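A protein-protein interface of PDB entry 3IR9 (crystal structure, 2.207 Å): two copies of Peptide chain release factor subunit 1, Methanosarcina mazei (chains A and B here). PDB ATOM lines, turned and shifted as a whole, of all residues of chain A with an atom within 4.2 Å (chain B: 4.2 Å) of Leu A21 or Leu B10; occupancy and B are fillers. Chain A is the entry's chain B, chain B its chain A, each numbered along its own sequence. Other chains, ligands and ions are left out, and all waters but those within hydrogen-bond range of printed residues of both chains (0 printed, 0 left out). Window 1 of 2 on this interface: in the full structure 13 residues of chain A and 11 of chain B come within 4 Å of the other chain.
OE2 of Glu A25 sits at hydrogen-bond distance from N of Asp B6 (3.3 Å).
The side-chain carboxylate (OD2) of Asp B6 sits at hydrogen-bond distance from the side-chain hydroxyl (OG) of Ser B8, 2.8 Å away.
The side-chain carboxylate (OD1) of Asp B6 is in hydrogen-bond range of the backbone NH (N) of Gly B9 (3.3 Å).
N of Leu B10 sits at hydrogen-bond distance from OD1 of Asp B6.
N of Ser B11 is in hydrogen-bond range of OD1 of Asp B6 (2.8 Å).
The backbone carbonyl oxygen (O) of Gly A18 sits at hydrogen-bond distance from the side-chain amide nitrogen (NE2) of Gln A22, 3.0 Å away.
Among the printed residues, merely in contact across the chains: Ala A17 with Val B14 (3.8 Å), Gly A18 with Val B14 (3.6 Å), Leu A21 with Leu B10 (3.9 Å), Leu A21 with Val B14 (3.5 Å) and Glu A25 with Ser B11 (3.5 Å).
Of chain B, only Leu B10 (3.9 Å) and Val B14 (3.5 Å) come within 4 Å of Leu A21.
Of the printed residues of chain A, Ser B11 touches Glu A25.
Of the printed residues of chain B, Glu A25 touches Asp B6 and Ser B11.
Of the printed residues of chain A, Val B14 touches Ala A17 (3.8 Å), Gly A18 (3.6 Å) and Leu A21 (3.5 Å).
Of the printed residues of chain B, Gly A18 touches Val B14 (3.6 Å).
Of the printed residues of chain A, Asp B6 touches Glu A25.
The nearest residue of chain B that does not touch Leu A21 is Ser B11 (4.1 Å).
Of the 9 printed residues of chain A, 4 touch a printed residue of chain B.
Printed residues of chain A that touch a printed residue of chain B: Ala A17, Gly A18, Leu A21 and Glu A25.
Hydrophobic or aromatic side chains of chain A within 4 Å of the printed part of chain B: Ala A17 and Leu A21.
Among the printed residues, 6 pairs touch across the chains.
Among the printed residues, no Asp or Glu carboxylate lies within 4 Å of a Lys or Arg side-chain nitrogen of the other chain.
No position is printed for both chains.
Of the 6 pairs that touch across the chains among the printed residues, none has its exchanged pair printed and touching as well.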
ATOM      1  N   ALA A  17       2.310 -12.171  -8.990  1.00  0.00           N
ATOM      2  CA  ALA A  17       3.334 -13.200  -9.118  1.00  0.00           C
ATOM      3  C   ALA A  17       4.147 -12.972 -10.384  1.00  0.00           C
ATOM      4  O   ALA A  17       5.322 -13.328 -10.451  1.00  0.00           O
ATOM      5  CB  ALA A  17       2.706 -14.579  -9.126  1.00  0.00           C
ATOM      6  N   GLY A  18       3.509 -12.371 -11.387  1.00  0.00           N
ATOM      7  CA  GLY A  18       4.183 -12.008 -12.619  1.00  0.00           C
ATOM      8  C   GLY A  18       5.096 -10.819 -12.407  1.00  0.00           C
ATOM      9  O   GLY A  18       5.977 -10.551 -13.225  1.00  0.00           O
ATOM     10  N   GLU A  19       4.881 -10.106 -11.303  1.00  0.00           N
ATOM     11  CA  GLU A  19       5.704  -8.952 -10.940  1.00  0.00           C
ATOM     12  C   GLU A  19       6.940  -9.408 -10.178  1.00  0.00           C
ATOM     13  O   GLU A  19       8.054  -8.972 -10.460  1.00  0.00           O
ATOM     14  CB  GLU A  19       4.901  -7.963 -10.087  1.00  0.00           C
ATOM     15  CG  GLU A  19       5.647  -6.680  -9.720  1.00  0.00           C
ATOM     16  CD  GLU A  19       5.653  -5.648 -10.843  1.00  0.00           C
ATOM     17  OE1 GLU A  19       6.062  -5.988 -11.974  1.00  0.00           O
ATOM     18  OE2 GLU A  19       5.251  -4.492 -10.589  1.00  0.00           O
ATOM     19  N   LYS A  20       6.732 -10.296  -9.211  1.00  0.00           N
ATOM     20  CA  LYS A  20       7.827 -10.871  -8.440  1.00  0.00           C
ATOM     21  C   LYS A  20       8.830 -11.582  -9.355  1.00  0.00           C
ATOM     22  O   LYS A  20      10.040 -11.430  -9.183  1.00  0.00           O
ATOM     23  CB  LYS A  20       7.269 -11.829  -7.383  1.00  0.00           C
ATOM     24  CG  LYS A  20       5.827 -11.508  -7.023  1.00  0.00           C
ATOM     25  CD  LYS A  20       5.374 -12.098  -5.700  1.00  0.00           C
ATOM     26  CE  LYS A  20       3.934 -11.675  -5.412  1.00  0.00           C
ATOM     27  NZ  LYS A  20       3.530 -11.810  -3.982  1.00  0.00           N
ATOM     28  N   LEU A  21       8.330 -12.337 -10.334  1.00  0.00           N
ATOM     29  CA  LEU A  21       9.196 -13.082 -11.256  1.00  0.00           C
ATOM     30  C   LEU A  21       9.839 -12.189 -12.329  1.00  0.00           C
ATOM     31  O   LEU A  21      10.901 -12.519 -12.864  1.00  0.00           O
ATOM     32  CB  LEU A  21       8.448 -14.255 -11.905  1.00  0.00           C
ATOM     33  CG  LEU A  21       8.016 -15.444 -11.034  1.00  0.00           C
ATOM     34  CD1 LEU A  21       7.181 -16.406 -11.856  1.00  0.00           C
ATOM     35  CD2 LEU A  21       9.198 -16.181 -10.409  1.00  0.00           C
ATOM     36  N   GLN A  22       9.209 -11.063 -12.645  1.00  0.00           N
ATOM     37  CA  GLN A  22       9.856 -10.084 -13.505  1.00  0.00           C
ATOM     38  C   GLN A  22      10.942  -9.364 -12.713  1.00  0.00           C
ATOM     39  O   GLN A  22      12.024  -9.095 -13.234  1.00  0.00           O
ATOM     40  CB  GLN A  22       8.843  -9.098 -14.091  1.00  0.00           C
ATOM     41  CG  GLN A  22       8.267  -9.534 -15.436  1.00  0.00           C
ATOM     42  CD  GLN A  22       7.004  -8.784 -15.819  1.00  0.00           C
ATOM     43  OE1 GLN A  22       6.529  -8.884 -16.951  1.00  0.00           O
ATOM     44  NE2 GLN A  22       6.451  -8.033 -14.875  1.00  0.00           N
ATOM     45  N   ASP A  23      10.648  -9.062 -11.449  1.00  0.00           N
ATOM     46  CA  ASP A  23      11.650  -8.542 -10.524  1.00  0.00           C
ATOM     47  C   ASP A  23      12.925  -9.365 -10.665  1.00  0.00           C
ATOM     48  O   ASP A  23      14.016  -8.819 -10.832  1.00  0.00           O
ATOM     49  CB  ASP A  23      11.156  -8.641  -9.069  1.00  0.00           C
ATOM     50  CG  ASP A  23      10.119  -7.578  -8.711  1.00  0.00           C
ATOM     51  OD1 ASP A  23      10.162  -6.484  -9.312  1.00  0.00           O
ATOM     52  OD2 ASP A  23       9.274  -7.834  -7.814  1.00  0.00           O
ATOM     53  N   LEU A  24      12.758 -10.686 -10.609  1.00  0.00           N
ATOM     54  CA  LEU A  24      13.870 -11.637 -10.583  1.00  0.00           C
ATOM     55  C   LEU A  24      14.585 -11.773 -11.920  1.00  0.00           C
ATOM     56  O   LEU A  24      15.816 -11.741 -11.977  1.00  0.00           O
ATOM     57  CB  LEU A  24      13.384 -13.012 -10.116  1.00  0.00           C
ATOM     58  CG  LEU A  24      13.140 -13.215  -8.617  1.00  0.00           C
ATOM     59  CD1 LEU A  24      12.844 -14.678  -8.305  1.00  0.00           C
ATOM     60  CD2 LEU A  24      14.334 -12.737  -7.811  1.00  0.00           C
ATOM     61  N   GLU A  25      13.811 -11.938 -12.989  1.00  0.00           N
ATOM     62  CA  GLU A  25      14.371 -12.099 -14.327  1.00  0.00           C
ATOM     63  C   GLU A  25      15.331 -10.965 -14.651  1.00  0.00           C
ATOM     64  O   GLU A  25      16.302 -11.150 -15.390  1.00  0.00           O
ATOM     65  CB  GLU A  25      13.259 -12.168 -15.378  1.00  0.00           C
ATOM     66  CG  GLU A  25      12.654 -13.555 -15.565  1.00  0.00           C
ATOM     67  CD  GLU A  25      13.548 -14.485 -16.371  1.00  0.00           C
ATOM     68  OE1 GLU A  25      14.582 -14.017 -16.897  1.00  0.00           O
ATOM     69  OE2 GLU A  25      13.210 -15.685 -16.480  1.00  0.00           O
ATOM     70  N   ASP B   6      15.065 -18.196 -15.421  1.00  0.00           N
ATOM     71  CA  ASP B   6      14.332 -19.341 -14.873  1.00  0.00           C
ATOM     72  C   ASP B   6      14.347 -20.573 -15.772  1.00  0.00           C
ATOM     73  O   ASP B   6      14.338 -20.460 -17.000  1.00  0.00           O
ATOM     74  CB  ASP B   6      12.887 -18.967 -14.554  1.00  0.00           C
ATOM     75  CG  ASP B   6      12.122 -20.110 -13.912  1.00  0.00           C
ATOM     76  OD1 ASP B   6      10.956 -20.336 -14.300  1.00  0.00           O
ATOM     77  OD2 ASP B   6      12.695 -20.791 -13.031  1.00  0.00           O
ATOM     78  N   SER B   8      13.214 -23.913 -13.961  1.00  0.00           N
ATOM     79  CA  SER B   8      12.265 -24.775 -13.270  1.00  0.00           C
ATOM     80  C   SER B   8      10.873 -24.579 -13.849  1.00  0.00           C
ATOM     81  O   SER B   8       9.922 -25.243 -13.441  1.00  0.00           O
ATOM     82  CB  SER B   8      12.246 -24.438 -11.786  1.00  0.00           C
ATOM     83  OG  SER B   8      12.001 -23.054 -11.607  1.00  0.00           O
ATOM     84  N   GLY B   9      10.760 -23.641 -14.784  1.00  0.00           N
ATOM     85  CA  GLY B   9       9.524 -23.413 -15.507  1.00  0.00           C
ATOM     86  C   GLY B   9       8.394 -22.834 -14.683  1.00  0.00           C
ATOM     87  O   GLY B   9       7.237 -23.208 -14.874  1.00  0.00           O
ATOM     88  N   LEU B  10       8.718 -21.932 -13.760  1.00  0.00           N
ATOM     89  CA  LEU B  10       7.687 -21.193 -13.038  1.00  0.00           C
ATOM     90  C   LEU B  10       7.352 -19.950 -13.844  1.00  0.00           C
ATOM     91  O   LEU B  10       6.200 -19.518 -13.904  1.00  0.00           O
ATOM     92  CB  LEU B  10       8.151 -20.803 -11.636  1.00  0.00           C
ATOM     93  CG  LEU B  10       7.065 -20.750 -10.553  1.00  0.00           C
ATOM     94  CD1 LEU B  10       5.786 -20.106 -11.062  1.00  0.00           C
ATOM     95  CD2 LEU B  10       6.766 -22.142 -10.028  1.00  0.00           C
ATOM     96  N   SER B  11       8.377 -19.378 -14.467  1.00  0.00           N
ATOM     97  CA  SER B  11       8.183 -18.283 -15.399  1.00  0.00           C
ATOM     98  C   SER B  11       7.113 -18.680 -16.398  1.00  0.00           C
ATOM     99  O   SER B  11       6.105 -17.996 -16.526  1.00  0.00           O
ATOM    100  CB  SER B  11       9.484 -17.959 -16.131  1.00  0.00           C
ATOM    101  OG  SER B  11      10.447 -17.441 -15.234  1.00  0.00           O
ATOM    102  N   GLU B  12       7.335 -19.798 -17.085  1.00  0.00           N
ATOM    103  CA  GLU B  12       6.383 -20.319 -18.063  1.00  0.00           C
ATOM    104  C   GLU B  12       4.993 -20.551 -17.458  1.00  0.00           C
ATOM    105  O   GLU B  12       3.981 -20.338 -18.125  1.00  0.00           O
ATOM    106  CB  GLU B  12       6.908 -21.617 -18.682  1.00  0.00           C
ATOM    107  CG  GLU B  12       8.252 -21.470 -19.374  1.00  0.00           C
ATOM    108  CD  GLU B  12       8.205 -20.502 -20.541  1.00  0.00           C
ATOM    109  OE1 GLU B  12       9.277 -20.000 -20.943  1.00  0.00           O
ATOM    110  OE2 GLU B  12       7.096 -20.244 -21.058  1.00  0.00           O
ATOM    111  N   LEU B  13       4.945 -20.988 -16.201  1.00  0.00           N
ATOM    112  CA  LEU B  13       3.667 -21.206 -15.526  1.00  0.00           C
ATOM    113  C   LEU B  13       2.956 -19.886 -15.270  1.00  0.00           C
ATOM    114  O   LEU B  13       1.889 -19.630 -15.825  1.00  0.00           O
ATOM    115  CB  LEU B  13       3.858 -21.969 -14.213  1.00  0.00           C
ATOM    116  CG  LEU B  13       4.144 -23.465 -14.363  1.00  0.00           C
ATOM    117  CD1 LEU B  13       4.126 -24.166 -13.017  1.00  0.00           C
ATOM    118  CD2 LEU B  13       3.135 -24.095 -15.305  1.00  0.00           C
ATOM    119  N   VAL B  14       3.553 -19.055 -14.423  1.00  0.00           N
ATOM    120  CA  VAL B  14       3.025 -17.724 -14.159  1.00  0.00           C
ATOM    121  C   VAL B  14       2.768 -16.997 -15.469  1.00  0.00           C
ATOM    122  O   VAL B  14       1.765 -16.297 -15.624  1.00  0.00           O
ATOM    123  CB  VAL B  14       4.000 -16.903 -13.299  1.00  0.00           C
ATOM    124  CG1 VAL B  14       3.942 -15.426 -13.672  1.00  0.00           C
ATOM    125  CG2 VAL B  14       3.702 -17.111 -11.820  1.00  0.00           C
